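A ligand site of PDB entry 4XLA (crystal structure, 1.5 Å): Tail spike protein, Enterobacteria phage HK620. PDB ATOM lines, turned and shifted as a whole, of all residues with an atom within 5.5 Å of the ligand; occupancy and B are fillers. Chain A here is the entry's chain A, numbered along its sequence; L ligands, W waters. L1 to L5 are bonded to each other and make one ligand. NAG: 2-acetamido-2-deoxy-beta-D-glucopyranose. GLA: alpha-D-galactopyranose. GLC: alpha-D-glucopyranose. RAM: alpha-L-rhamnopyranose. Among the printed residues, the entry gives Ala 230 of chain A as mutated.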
ATOM      1  N   GLY A 102      -5.823   2.542  22.810  1.00  0.00           N
ATOM      2  CA  GLY A 102      -6.012   1.382  21.924  1.00  0.00           C
ATOM      3  C   GLY A 102      -4.842   0.409  22.032  1.00  0.00           C
ATOM      4  O   GLY A 102      -4.967  -0.730  21.537  1.00  0.00           O
ATOM      5  N   HIS A 103      -3.750   0.758  22.724  1.00  0.00           N
ATOM      6  CA  HIS A 103      -2.560  -0.060  22.842  1.00  0.00           C
ATOM      7  C   HIS A 103      -2.397  -0.475  24.272  1.00  0.00           C
ATOM      8  O   HIS A 103      -1.339  -0.893  24.676  1.00  0.00           O
ATOM      9  CB  HIS A 103      -1.320   0.732  22.377  1.00  0.00           C
ATOM     10  CG  HIS A 103      -1.416   1.285  21.001  1.00  0.00           C
ATOM     11  ND1 HIS A 103      -1.037   0.566  19.892  1.00  0.00           N
ATOM     12  CD2 HIS A 103      -1.884   2.455  20.524  1.00  0.00           C
ATOM     13  CE1 HIS A 103      -1.244   1.277  18.811  1.00  0.00           C
ATOM     14  NE2 HIS A 103      -1.762   2.431  19.164  1.00  0.00           N
ATOM     15  N   SER A 104      -3.459  -0.303  25.109  1.00  0.00           N
ATOM     16  CA  SER A 104      -3.346  -0.577  26.569  1.00  0.00           C
ATOM     17  C   SER A 104      -2.193   0.216  27.142  1.00  0.00           C
ATOM     18  O   SER A 104      -1.555  -0.188  28.099  1.00  0.00           O
ATOM     19  CB  SER A 104      -3.174  -2.055  26.847  1.00  0.00           C
ATOM     20  OG  SER A 104      -4.241  -2.719  26.193  1.00  0.00           O
ATOM     21  N   GLN A 133       0.961  -1.707  27.920  1.00  0.00           N
ATOM     22  CA  GLN A 133       2.219  -1.327  27.269  1.00  0.00           C
ATOM     23  C   GLN A 133       2.676  -0.115  27.933  1.00  0.00           C
ATOM     24  O   GLN A 133       1.975   0.933  27.881  1.00  0.00           O
ATOM     25  CB  GLN A 133       1.992  -1.128  25.785  1.00  0.00           C
ATOM     26  CG  GLN A 133       1.530  -2.432  25.105  1.00  0.00           C
ATOM     27  CD  GLN A 133       1.622  -2.358  23.595  1.00  0.00           C
ATOM     28  OE1 GLN A 133       2.697  -2.196  22.997  1.00  0.00           O
ATOM     29  NE2 GLN A 133       0.507  -2.556  22.914  1.00  0.00           N
ATOM     30  N   PHE A 138       3.053   5.504  19.706  1.00  0.00           N
ATOM     31  CA  PHE A 138       1.939   5.818  18.761  1.00  0.00           C
ATOM     32  C   PHE A 138       1.145   6.968  19.356  1.00  0.00           C
ATOM     33  O   PHE A 138       1.058   7.111  20.551  1.00  0.00           O
ATOM     34  CB  PHE A 138       1.045   4.617  18.594  1.00  0.00           C
ATOM     35  CG  PHE A 138       1.721   3.388  17.926  1.00  0.00           C
ATOM     36  CD1 PHE A 138       2.012   3.382  16.572  1.00  0.00           C
ATOM     37  CD2 PHE A 138       1.992   2.265  18.667  1.00  0.00           C
ATOM     38  CE1 PHE A 138       2.587   2.209  15.989  1.00  0.00           C
ATOM     39  CE2 PHE A 138       2.516   1.115  18.117  1.00  0.00           C
ATOM     40  CZ  PHE A 138       2.823   1.103  16.778  1.00  0.00           C
ATOM     41  N   PRO A 143      -2.486   2.047  14.378  1.00  0.00           N
ATOM     42  CA  PRO A 143      -1.114   2.431  14.026  1.00  0.00           C
ATOM     43  C   PRO A 143      -0.979   3.000  12.617  1.00  0.00           C
ATOM     44  O   PRO A 143      -0.126   3.865  12.323  1.00  0.00           O
ATOM     45  CB  PRO A 143      -0.349   1.129  14.211  1.00  0.00           C
ATOM     46  CG  PRO A 143      -1.331   0.049  14.295  1.00  0.00           C
ATOM     47  CD  PRO A 143      -2.571   0.692  14.891  1.00  0.00           C
ATOM     48  N   LEU A 173      -1.746  -8.834  25.460  1.00  0.00           N
ATOM     49  CA  LEU A 173      -0.366  -8.363  25.046  1.00  0.00           C
ATOM     50  C   LEU A 173       0.176  -7.484  26.155  1.00  0.00           C
ATOM     51  O   LEU A 173      -0.558  -6.684  26.766  1.00  0.00           O
ATOM     52  CB  LEU A 173      -0.396  -7.490  23.757  1.00  0.00           C
ATOM     53  CG  LEU A 173      -0.842  -8.295  22.556  1.00  0.00           C
ATOM     54  CD1 LEU A 173      -1.204  -7.417  21.364  1.00  0.00           C
ATOM     55  CD2 LEU A 173       0.047  -9.446  22.169  1.00  0.00           C
ATOM     56  N   ASN A 175       3.901  -5.127  26.951  1.00  0.00           N
ATOM     57  CA  ASN A 175       5.131  -4.546  26.366  1.00  0.00           C
ATOM     58  C   ASN A 175       5.686  -3.560  27.424  1.00  0.00           C
ATOM     59  O   ASN A 175       4.953  -2.904  28.145  1.00  0.00           O
ATOM     60  CB  ASN A 175       4.837  -3.828  25.055  1.00  0.00           C
ATOM     61  CG  ASN A 175       6.065  -3.569  24.185  1.00  0.00           C
ATOM     62  OD1 ASN A 175       7.219  -3.941  24.467  1.00  0.00           O
ATOM     63  ND2 ASN A 175       5.793  -2.947  23.053  1.00  0.00           N
ATOM     64  N   THR A 198       4.852  -9.946  26.740  1.00  0.00           N
ATOM     65  CA  THR A 198       5.033 -10.443  25.387  1.00  0.00           C
ATOM     66  C   THR A 198       6.390  -9.985  24.839  1.00  0.00           C
ATOM     67  O   THR A 198       7.140 -10.791  24.244  1.00  0.00           O
ATOM     68  CB  THR A 198       3.928  -9.894  24.479  1.00  0.00           C
ATOM     69  OG1 THR A 198       2.622 -10.134  25.072  1.00  0.00           O
ATOM     70  CG2 THR A 198       3.987 -10.488  23.129  1.00  0.00           C
ATOM     71  N   TRP A 199       6.624  -8.679  24.962  1.00  0.00           N
ATOM     72  CA  TRP A 199       7.909  -8.041  24.572  1.00  0.00           C
ATOM     73  C   TRP A 199       8.372  -7.097  25.714  1.00  0.00           C
ATOM     74  O   TRP A 199       7.517  -6.659  26.515  1.00  0.00           O
ATOM     75  CB  TRP A 199       7.739  -7.183  23.343  1.00  0.00           C
ATOM     76  CG  TRP A 199       7.048  -7.855  22.157  1.00  0.00           C
ATOM     77  CD1 TRP A 199       7.539  -8.811  21.342  1.00  0.00           C
ATOM     78  CD2 TRP A 199       5.696  -7.620  21.737  1.00  0.00           C
ATOM     79  NE1 TRP A 199       6.638  -9.128  20.361  1.00  0.00           N
ATOM     80  CE2 TRP A 199       5.443  -8.480  20.635  1.00  0.00           C
ATOM     81  CE3 TRP A 199       4.680  -6.798  22.214  1.00  0.00           C
ATOM     82  CZ2 TRP A 199       4.222  -8.443  19.950  1.00  0.00           C
ATOM     83  CZ3 TRP A 199       3.454  -6.810  21.576  1.00  0.00           C
ATOM     84  CH2 TRP A 199       3.232  -7.638  20.481  1.00  0.00           C
ATOM     85  N   THR A 202       9.610  -2.918  21.592  1.00  0.00           N
ATOM     86  CA  THR A 202       9.407  -3.020  20.180  1.00  0.00           C
ATOM     87  C   THR A 202       9.805  -1.734  19.455  1.00  0.00           C
ATOM     88  O   THR A 202       9.630  -0.625  20.002  1.00  0.00           O
ATOM     89  CB  THR A 202       7.972  -3.328  19.794  1.00  0.00           C
ATOM     90  OG1 THR A 202       7.068  -2.263  20.186  1.00  0.00           O
ATOM     91  CG2 THR A 202       7.511  -4.593  20.531  1.00  0.00           C
ATOM     92  N   LEU A 203      10.429  -1.908  18.300  1.00  0.00           N
ATOM     93  CA  LEU A 203      10.959  -0.814  17.496  1.00  0.00           C
ATOM     94  C   LEU A 203      10.224  -0.755  16.204  1.00  0.00           C
ATOM     95  O   LEU A 203      10.157  -1.809  15.515  1.00  0.00           O
ATOM     96  CB  LEU A 203      12.466  -0.981  17.209  1.00  0.00           C
ATOM     97  CG  LEU A 203      13.323  -1.282  18.433  1.00  0.00           C
ATOM     98  CD1 LEU A 203      14.769  -1.451  17.924  1.00  0.00           C
ATOM     99  CD2 LEU A 203      13.190  -0.199  19.463  1.00  0.00           C
ATOM    100  N   GLY A 204       9.709   0.387  15.778  1.00  0.00           N
ATOM    101  CA  GLY A 204       9.059   0.456  14.496  1.00  0.00           C
ATOM    102  C   GLY A 204       7.651  -0.075  14.482  1.00  0.00           C
ATOM    103  O   GLY A 204       7.170  -0.715  15.447  1.00  0.00           O
ATOM    104  N   TRP A 205       7.052   0.009  13.310  1.00  0.00           N
ATOM    105  CA  TRP A 205       5.718  -0.554  13.077  1.00  0.00           C
ATOM    106  C   TRP A 205       5.600  -0.897  11.650  1.00  0.00           C
ATOM    107  O   TRP A 205       5.606   0.012  10.772  1.00  0.00           O
ATOM    108  CB  TRP A 205       4.542   0.340  13.501  1.00  0.00           C
ATOM    109  CG  TRP A 205       3.241  -0.277  13.162  1.00  0.00           C
ATOM    110  CD1 TRP A 205       2.687  -1.329  13.755  1.00  0.00           C
ATOM    111  CD2 TRP A 205       2.449   0.022  12.008  1.00  0.00           C
ATOM    112  NE1 TRP A 205       1.536  -1.708  13.092  1.00  0.00           N
ATOM    113  CE2 TRP A 205       1.352  -0.872  12.027  1.00  0.00           C
ATOM    114  CE3 TRP A 205       2.508   1.008  11.033  1.00  0.00           C
ATOM    115  CZ2 TRP A 205       0.352  -0.819  11.056  1.00  0.00           C
ATOM    116  CZ3 TRP A 205       1.539   1.071  10.080  1.00  0.00           C
ATOM    117  CH2 TRP A 205       0.456   0.145  10.098  1.00  0.00           C
ATOM    118  N   ASN A 206       5.581  -2.195  11.338  1.00  0.00           N
ATOM    119  CA  ASN A 206       5.419  -2.659   9.930  1.00  0.00           C
ATOM    120  C   ASN A 206       6.307  -1.997   8.941  1.00  0.00           C
ATOM    121  O   ASN A 206       5.904  -1.610   7.857  1.00  0.00           O
ATOM    122  CB  ASN A 206       3.958  -2.750   9.498  1.00  0.00           C
ATOM    123  CG  ASN A 206       3.170  -3.710  10.310  1.00  0.00           C
ATOM    124  OD1 ASN A 206       3.681  -4.424  11.172  1.00  0.00           O
ATOM    125  ND2 ASN A 206       1.842  -3.721  10.080  1.00  0.00           N
ATOM    126  N   ALA A 230       3.615 -16.313  24.380  1.00  0.00           N
ATOM    127  CA  ALA A 230       4.842 -16.190  23.626  1.00  0.00           C
ATOM    128  C   ALA A 230       5.574 -14.979  24.108  1.00  0.00           C
ATOM    129  O   ALA A 230       4.990 -13.963  24.493  1.00  0.00           O
ATOM    130  CB  ALA A 230       4.528 -15.991  22.152  1.00  0.00           C
ATOM    131  N   HIS A 231       6.890 -15.030  24.026  1.00  0.00           N
ATOM    132  CA  HIS A 231       7.661 -13.858  24.420  1.00  0.00           C
ATOM    133  C   HIS A 231       8.848 -13.665  23.515  1.00  0.00           C
ATOM    134  O   HIS A 231       9.611 -14.612  23.298  1.00  0.00           O
ATOM    135  CB  HIS A 231       8.172 -14.050  25.821  1.00  0.00           C
ATOM    136  CG  HIS A 231       9.133 -12.997  26.243  1.00  0.00           C
ATOM    137  ND1 HIS A 231       8.771 -11.903  27.002  1.00  0.00           N
ATOM    138  CD2 HIS A 231      10.473 -12.873  26.021  1.00  0.00           C
ATOM    139  CE1 HIS A 231       9.828 -11.134  27.171  1.00  0.00           C
ATOM    140  NE2 HIS A 231      10.860 -11.707  26.588  1.00  0.00           N
ATOM    141  N   SER A 232       9.038 -12.444  23.006  1.00  0.00           N
ATOM    142  CA  SER A 232      10.304 -12.059  22.354  1.00  0.00           C
ATOM    143  C   SER A 232      10.783 -10.711  22.894  1.00  0.00           C
ATOM    144  O   SER A 232      10.037  -9.751  22.941  1.00  0.00           O
ATOM    145  CB  SER A 232      10.137 -11.970  20.856  1.00  0.00           C
ATOM    146  OG  SER A 232       9.918 -13.320  20.359  1.00  0.00           O
ATOM    147  N   TYR A 235      11.576  -6.800  19.597  1.00  0.00           N
ATOM    148  CA  TYR A 235      11.041  -7.034  18.239  1.00  0.00           C
ATOM    149  C   TYR A 235      11.386  -5.818  17.371  1.00  0.00           C
ATOM    150  O   TYR A 235      10.913  -4.691  17.642  1.00  0.00           O
ATOM    151  CB  TYR A 235       9.540  -7.274  18.346  1.00  0.00           C
ATOM    152  CG  TYR A 235       8.820  -7.901  17.173  1.00  0.00           C
ATOM    153  CD1 TYR A 235       8.551  -7.217  16.028  1.00  0.00           C
ATOM    154  CD2 TYR A 235       8.338  -9.215  17.241  1.00  0.00           C
ATOM    155  CE1 TYR A 235       7.835  -7.792  14.981  1.00  0.00           C
ATOM    156  CE2 TYR A 235       7.612  -9.760  16.217  1.00  0.00           C
ATOM    157  CZ  TYR A 235       7.367  -9.074  15.099  1.00  0.00           C
ATOM    158  OH  TYR A 235       6.623  -9.623  14.091  1.00  0.00           O
ATOM    159  N   ASN A 237      11.133  -3.928  14.147  1.00  0.00           N
ATOM    160  CA  ASN A 237      10.189  -3.866  13.049  1.00  0.00           C
ATOM    161  C   ASN A 237      10.305  -2.538  12.252  1.00  0.00           C
ATOM    162  O   ASN A 237       9.389  -2.053  11.648  1.00  0.00           O
ATOM    163  CB  ASN A 237       8.739  -4.081  13.555  1.00  0.00           C
ATOM    164  CG  ASN A 237       7.838  -4.629  12.451  1.00  0.00           C
ATOM    165  OD1 ASN A 237       8.276  -5.003  11.374  1.00  0.00           O
ATOM    166  ND2 ASN A 237       6.540  -4.724  12.759  1.00  0.00           N
ATOM    167  N   CYS A 260      12.101 -15.983  23.167  1.00  0.00           N
ATOM    168  CA  CYS A 260      13.109 -15.635  22.191  1.00  0.00           C
ATOM    169  C   CYS A 260      13.743 -14.285  22.573  1.00  0.00           C
ATOM    170  O   CYS A 260      13.011 -13.388  23.105  1.00  0.00           O
ATOM    171  CB  CYS A 260      12.496 -15.551  20.817  1.00  0.00           C
ATOM    172  SG  CYS A 260      13.744 -15.339  19.507  1.00  0.00           S
ATOM    173  N   GLU A 263      13.872 -10.439  17.676  1.00  0.00           N
ATOM    174  CA  GLU A 263      13.341 -10.720  16.350  1.00  0.00           C
ATOM    175  C   GLU A 263      13.716  -9.590  15.420  1.00  0.00           C
ATOM    176  O   GLU A 263      13.492  -8.419  15.716  1.00  0.00           O
ATOM    177  CB  GLU A 263      11.851 -11.016  16.273  1.00  0.00           C
ATOM    178  CG  GLU A 263      11.408 -12.063  17.303  1.00  0.00           C
ATOM    179  CD  GLU A 263      10.164 -12.820  16.921  1.00  0.00           C
ATOM    180  OE1 GLU A 263       9.676 -12.675  15.790  1.00  0.00           O
ATOM    181  OE2 GLU A 263       9.643 -13.571  17.787  1.00  0.00           O
ATOM    182  N   HIS A 265      12.958  -8.117  11.796  1.00  0.00           N
ATOM    183  CA  HIS A 265      11.825  -8.219  10.884  1.00  0.00           C
ATOM    184  C   HIS A 265      11.869  -7.257   9.705  1.00  0.00           C
ATOM    185  O   HIS A 265      10.952  -7.240   8.913  1.00  0.00           O
ATOM    186  CB  HIS A 265      10.520  -8.064  11.660  1.00  0.00           C
ATOM    187  CG  HIS A 265      10.075  -9.315  12.314  1.00  0.00           C
ATOM    188  ND1 HIS A 265       9.426 -10.326  11.634  1.00  0.00           N
ATOM    189  CD2 HIS A 265      10.154  -9.715  13.578  1.00  0.00           C
ATOM    190  CE1 HIS A 265       9.184 -11.321  12.444  1.00  0.00           C
ATOM    191  NE2 HIS A 265       9.669 -11.003  13.626  1.00  0.00           N
ATOM    192  N   TYR A 284      14.665 -14.714  15.839  1.00  0.00           N
ATOM    193  CA  TYR A 284      14.019 -14.849  14.558  1.00  0.00           C
ATOM    194  C   TYR A 284      14.557 -13.806  13.562  1.00  0.00           C
ATOM    195  O   TYR A 284      14.781 -12.657  13.914  1.00  0.00           O
ATOM    196  CB  TYR A 284      12.522 -14.656  14.672  1.00  0.00           C
ATOM    197  CG  TYR A 284      11.776 -15.808  15.307  1.00  0.00           C
ATOM    198  CD1 TYR A 284      11.650 -15.940  16.687  1.00  0.00           C
ATOM    199  CD2 TYR A 284      11.307 -16.836  14.510  1.00  0.00           C
ATOM    200  CE1 TYR A 284      10.983 -17.049  17.230  1.00  0.00           C
ATOM    201  CE2 TYR A 284      10.616 -17.940  15.053  1.00  0.00           C
ATOM    202  CZ  TYR A 284      10.520 -18.050  16.398  1.00  0.00           C
ATOM    203  OH  TYR A 284       9.841 -19.154  16.948  1.00  0.00           O
ATOM    204  N   VAL A 286      13.087 -12.866  10.003  1.00  0.00           N
ATOM    205  CA  VAL A 286      11.866 -13.244   9.234  1.00  0.00           C
ATOM    206  C   VAL A 286      11.414 -12.001   8.451  1.00  0.00           C
ATOM    207  O   VAL A 286      11.306 -10.910   9.022  1.00  0.00           O
ATOM    208  CB  VAL A 286      10.798 -13.731  10.214  1.00  0.00           C
ATOM    209  CG1 VAL A 286       9.448 -13.971   9.527  1.00  0.00           C
ATOM    210  CG2 VAL A 286      11.194 -15.018  10.834  1.00  0.00           C
ATOM    211  N   HIS A 288       7.968 -10.992   7.106  1.00  0.00           N
ATOM    212  CA  HIS A 288       6.537 -11.264   7.045  1.00  0.00           C
ATOM    213  C   HIS A 288       5.917 -10.341   5.981  1.00  0.00           C
ATOM    214  O   HIS A 288       6.041  -9.114   6.088  1.00  0.00           O
ATOM    215  CB  HIS A 288       5.871 -10.884   8.337  1.00  0.00           C
ATOM    216  CG  HIS A 288       5.997 -11.854   9.433  1.00  0.00           C
ATOM    217  ND1 HIS A 288       5.867 -13.207   9.267  1.00  0.00           N
ATOM    218  CD2 HIS A 288       6.285 -11.675  10.746  1.00  0.00           C
ATOM    219  CE1 HIS A 288       6.005 -13.814  10.436  1.00  0.00           C
ATOM    220  NE2 HIS A 288       6.255 -12.906  11.346  1.00  0.00           N
ATOM    221  N   ALA A 290       2.979  -9.619   5.847  1.00  0.00           N
ATOM    222  CA  ALA A 290       2.038  -8.765   6.583  1.00  0.00           C
ATOM    223  C   ALA A 290       2.671  -7.501   7.172  1.00  0.00           C
ATOM    224  O   ALA A 290       1.940  -6.597   7.659  1.00  0.00           O
ATOM    225  CB  ALA A 290       1.355  -9.550   7.701  1.00  0.00           C
ATOM    226  N   GLU A 291       4.005  -7.467   7.267  1.00  0.00           N
ATOM    227  CA  GLU A 291       4.751  -6.356   7.856  1.00  0.00           C
ATOM    228  C   GLU A 291       5.514  -5.534   6.887  1.00  0.00           C
ATOM    229  O   GLU A 291       6.348  -4.705   7.253  1.00  0.00           O
ATOM    230  CB  GLU A 291       5.726  -6.856   8.954  1.00  0.00           C
ATOM    231  CG  GLU A 291       4.968  -7.509  10.119  1.00  0.00           C
ATOM    232  CD  GLU A 291       5.849  -8.046  11.220  1.00  0.00           C
ATOM    233  OE1 GLU A 291       7.017  -8.344  10.928  1.00  0.00           O
ATOM    234  OE2 GLU A 291       5.394  -8.106  12.355  1.00  0.00           O
ATOM    235  N   ASN A 362       3.700 -19.039  10.106  1.00  0.00           N
ATOM    236  CA  ASN A 362       2.921 -19.118  11.321  1.00  0.00           C
ATOM    237  C   ASN A 362       1.747 -20.071  11.225  1.00  0.00           C
ATOM    238  O   ASN A 362       1.276 -20.516  12.263  1.00  0.00           O
ATOM    239  CB  ASN A 362       2.450 -17.701  11.761  1.00  0.00           C
ATOM    240  CG  ASN A 362       3.604 -16.879  12.364  1.00  0.00           C
ATOM    241  OD1 ASN A 362       4.682 -17.419  12.663  1.00  0.00           O
ATOM    242  ND2 ASN A 362       3.372 -15.621  12.555  1.00  0.00           N
HETATM  243  C1  NAG L   1       7.139 -15.245  17.021  1.00  0.00           C
HETATM  244  C2  NAG L   1       6.519 -13.840  17.121  1.00  0.00           C
HETATM  245  C3  NAG L   1       5.470 -13.719  16.014  1.00  0.00           C
HETATM  246  C4  NAG L   1       6.217 -13.930  14.740  1.00  0.00           C
HETATM  247  C5  NAG L   1       7.047 -15.277  14.664  1.00  0.00           C
HETATM  248  C6  NAG L   1       8.022 -15.299  13.509  1.00  0.00           C
HETATM  249  C7  NAG L   1       6.198 -12.582  19.269  1.00  0.00           C
HETATM  250  C8  NAG L   1       5.620 -12.598  20.638  1.00  0.00           C
HETATM  251  N2  NAG L   1       5.969 -13.664  18.432  1.00  0.00           N
HETATM  252  O1  NAG L   1       8.108 -15.442  18.017  1.00  0.00           O
HETATM  253  O3  NAG L   1       4.788 -12.522  16.102  1.00  0.00           O
HETATM  254  O4  NAG L   1       5.339 -13.874  13.612  1.00  0.00           O
HETATM  255  O5  NAG L   1       7.813 -15.423  15.808  1.00  0.00           O
HETATM  256  O6  NAG L   1       8.963 -14.216  13.541  1.00  0.00           O
HETATM  257  O7  NAG L   1       6.883 -11.615  18.893  1.00  0.00           O
HETATM  258  C1  GLA L   2       3.390 -12.554  15.691  1.00  0.00           C
HETATM  259  C2  GLA L   2       3.015 -11.154  15.190  1.00  0.00           C
HETATM  260  C3  GLA L   2       3.073 -10.153  16.390  1.00  0.00           C
HETATM  261  C4  GLA L   2       2.361 -10.616  17.635  1.00  0.00           C
HETATM  262  C5  GLA L   2       2.837 -12.017  17.974  1.00  0.00           C
HETATM  263  C6  GLA L   2       2.138 -12.613  19.197  1.00  0.00           C
HETATM  264  O2  GLA L   2       3.891 -10.830  14.129  1.00  0.00           O
HETATM  265  O3  GLA L   2       2.542  -8.970  15.811  1.00  0.00           O
HETATM  266  O4  GLA L   2       0.926 -10.687  17.313  1.00  0.00           O
HETATM  267  O5  GLA L   2       2.747 -12.919  16.869  1.00  0.00           O
HETATM  268  O6  GLA L   2       2.195 -11.644  20.281  1.00  0.00           O
HETATM  269  C1  GLC L   3       0.146 -10.056  18.345  1.00  0.00           C
HETATM  270  C2  GLC L   3      -1.314 -10.496  18.075  1.00  0.00           C
HETATM  271  C3  GLC L   3      -1.878  -9.905  16.807  1.00  0.00           C
HETATM  272  C4  GLC L   3      -1.714  -8.415  16.856  1.00  0.00           C
HETATM  273  C5  GLC L   3      -0.201  -8.083  16.981  1.00  0.00           C
HETATM  274  C6  GLC L   3       0.134  -6.612  17.014  1.00  0.00           C
HETATM  275  O2  GLC L   3      -1.454 -11.918  18.105  1.00  0.00           O
HETATM  276  O3  GLC L   3      -3.293 -10.244  16.810  1.00  0.00           O
HETATM  277  O4  GLC L   3      -2.203  -7.890  15.679  1.00  0.00           O
HETATM  278  O5  GLC L   3       0.210  -8.642  18.218  1.00  0.00           O
HETATM  279  O6  GLC L   3      -0.615  -5.988  18.090  1.00  0.00           O
HETATM  280  C1  NAG L   4       3.526  -7.936  15.491  1.00  0.00           C
HETATM  281  C2  NAG L   4       2.863  -6.972  14.493  1.00  0.00           C
HETATM  282  C3  NAG L   4       3.757  -5.739  14.349  1.00  0.00           C
HETATM  283  C4  NAG L   4       4.306  -5.182  15.659  1.00  0.00           C
HETATM  284  C5  NAG L   4       4.948  -6.294  16.407  1.00  0.00           C
HETATM  285  C6  NAG L   4       5.498  -5.886  17.727  1.00  0.00           C
HETATM  286  C7  NAG L   4       1.499  -7.854  12.664  1.00  0.00           C
HETATM  287  C8  NAG L   4       1.492  -8.585  11.346  1.00  0.00           C
HETATM  288  N2  NAG L   4       2.673  -7.630  13.215  1.00  0.00           N
HETATM  289  O3  NAG L   4       2.969  -4.740  13.702  1.00  0.00           O
HETATM  290  O4  NAG L   4       5.344  -4.239  15.276  1.00  0.00           O
HETATM  291  O5  NAG L   4       3.961  -7.301  16.707  1.00  0.00           O
HETATM  292  O6  NAG L   4       4.485  -5.355  18.571  1.00  0.00           O
HETATM  293  O7  NAG L   4       0.453  -7.518  13.175  1.00  0.00           O
HETATM  294  C1  RAM L   5      -1.486  -4.983  17.590  1.00  0.00           C
HETATM  295  C2  RAM L   5      -2.317  -4.508  18.795  1.00  0.00           C
HETATM  296  C3  RAM L   5      -1.537  -3.584  19.677  1.00  0.00           C
HETATM  297  C4  RAM L   5      -0.768  -2.563  18.932  1.00  0.00           C
HETATM  298  C5  RAM L   5       0.089  -3.208  17.850  1.00  0.00           C
HETATM  299  C6  RAM L   5       0.841  -2.170  17.036  1.00  0.00           C
HETATM  300  O2  RAM L   5      -3.352  -3.694  18.246  1.00  0.00           O
HETATM  301  O3  RAM L   5      -2.470  -2.953  20.635  1.00  0.00           O
HETATM  302  O4  RAM L   5       0.017  -1.951  19.961  1.00  0.00           O
HETATM  303  O5  RAM L   5      -0.775  -3.932  16.934  1.00  0.00           O
HETATM  304  O   HOH W   1       2.679  -1.558  20.392  1.00  0.00           O
HETATM  305  O   HOH W   2       4.811  -1.824  16.313  1.00  0.00           O
HETATM  306  O   HOH W   3      -2.588 -12.384  20.689  1.00  0.00           O
HETATM  307  O   HOH W   4       7.111 -18.410  15.521  1.00  0.00           O
HETATM  308  O   HOH W   5       2.708 -12.327  12.066  1.00  0.00           O
HETATM  309  O   HOH W   6       7.901 -18.068  18.715  1.00  0.00           O
HETATM  310  O   HOH W   7      -4.971  -3.301  20.754  1.00  0.00           O
HETATM  311  O   HOH W   8      -0.007 -13.496  16.366  1.00  0.00           O
HETATM  312  O   HOH W   9       4.705  -2.657  19.073  1.00  0.00           O
HETATM  313  O   HOH W  10       1.437 -13.257  22.290  1.00  0.00           O
HETATM  314  O   HOH W  11      -0.316  -5.351  11.284  1.00  0.00           O
HETATM  315  O   HOH W  12      -1.705  -8.939  13.400  1.00  0.00           O
HETATM  316  O   HOH W  13       0.000  -4.098  14.071  1.00  0.00           O
HETATM  317  O   HOH W  14      -3.037  -2.346  15.730  1.00  0.00           O
HETATM  318  O   HOH W  15       3.948 -15.915  18.876  1.00  0.00           O
HETATM  319  O   HOH W  16       8.191 -15.492  20.783  1.00  0.00           O
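O of Gly 102 is in hydrogen-bond range of O3 of RAM L5 (3.5 Å).
The side-chain amide nitrogen of Gln 133 lies within hydrogen-bond range of an oxygen (O4) of RAM L5, 3.1 Å away.
OD1 of Asn 206 is in hydrogen-bond range of O3 of NAG L4, at 2.6 Å.
The side-chain carboxylate of Glu 291 is in hydrogen-bond range of a nitrogen (N2) of NAG L4 (2.9 Å).
A ring nitrogen (NE2) of His 265 lies close to an oxygen (O6) of NAG L1 (3.3 Å).
The side-chain hydroxyl of Tyr 235 sits at hydrogen-bond distance from an oxygen (O2) of GLA L2 (3.0 Å).
OE2 of Glu 263 sits at hydrogen-bond distance from O1 of NAG L1.
NE1 of Trp 205 sits at hydrogen-bond distance from O3 of NAG L4.
The side-chain amide nitrogen (ND2) of Asn 362 lies within hydrogen-bond range of an oxygen (O4) of NAG L1, at 2.8 Å.
The indole nitrogen (NE1) of Trp 199 sits at hydrogen-bond distance from an oxygen (O7) of NAG L1 (2.9 Å).
A ring nitrogen (NE2) of His 288 sits at hydrogen-bond distance from an oxygen (O4) of NAG L1, at 2.6 Å.
ND2 of Asn 237 lies within hydrogen-bond range of O4 of NAG L4 (2.8 Å).
An oxygen (O4) of RAM L5 is in hydrogen-bond range of a ring nitrogen (ND1) of His 103 (2.7 Å).
OE1 of Gln 133 is in hydrogen-bond range of ND2 of Asn 175 (3.2 Å).
A ring nitrogen (ND1) of His 231 sits close to the backbone carbonyl oxygen (O) of Thr 198, at 3.4 Å.
O of Leu 203 lies within hydrogen-bond range of N of Asn 237, at 2.7 Å.
OE1 of Glu 291 sits at hydrogen-bond distance from ND1 of His 265 (3.2 Å).
OG1 of Thr 202 is in hydrogen-bond range of ND2 of Asn 175.
OE2 of Glu 263 is in hydrogen-bond range of OG of Ser 232 (2.6 Å).
The backbone NH (N) of Asn 206 sits close to the side-chain amide nitrogen (ND2) of Asn 237.
OH of Tyr 235 sits close to NE2 of His 265.
Merely in contact with the ligand: Tyr 284, Thr 198, Val 286, Leu 173, Ser 232, Thr 202, Ala 290, Phe 138, Ala 230 and Gly 204.
Hydrophobic or aromatic side chains within 4 Å of the ligand: His 103, Phe 138, Leu 173, Trp 199, Trp 205, Ala 230, Tyr 235, His 265, Tyr 284, Val 286, His 288 and Ala 290.
The nearest printed residue that does not touch the ligand is Pro 143 (4.1 Å).
Water W7 bridges O3 of RAM L5 (2.5 Å) and O of Gly 102 (2.7 Å).
Water W6 bridges an oxygen (O1) of NAG L1 and the side-chain hydroxyl (OH) of Tyr 284.
Water W9 lies within hydrogen-bond range of OG1 of Thr 202 and O6 of NAG L4.
Water W5 bridges O2 of GLA L2 and ND2 of Asn 362.
Water W11 lies within hydrogen-bond range of ND2 of Asn 206 (3.0 Å) and O7 of NAG L4 (3.0 Å).
Water W4 bridges O5 of NAG L1 (3.1 Å) and OH of Tyr 284 (3.2 Å).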
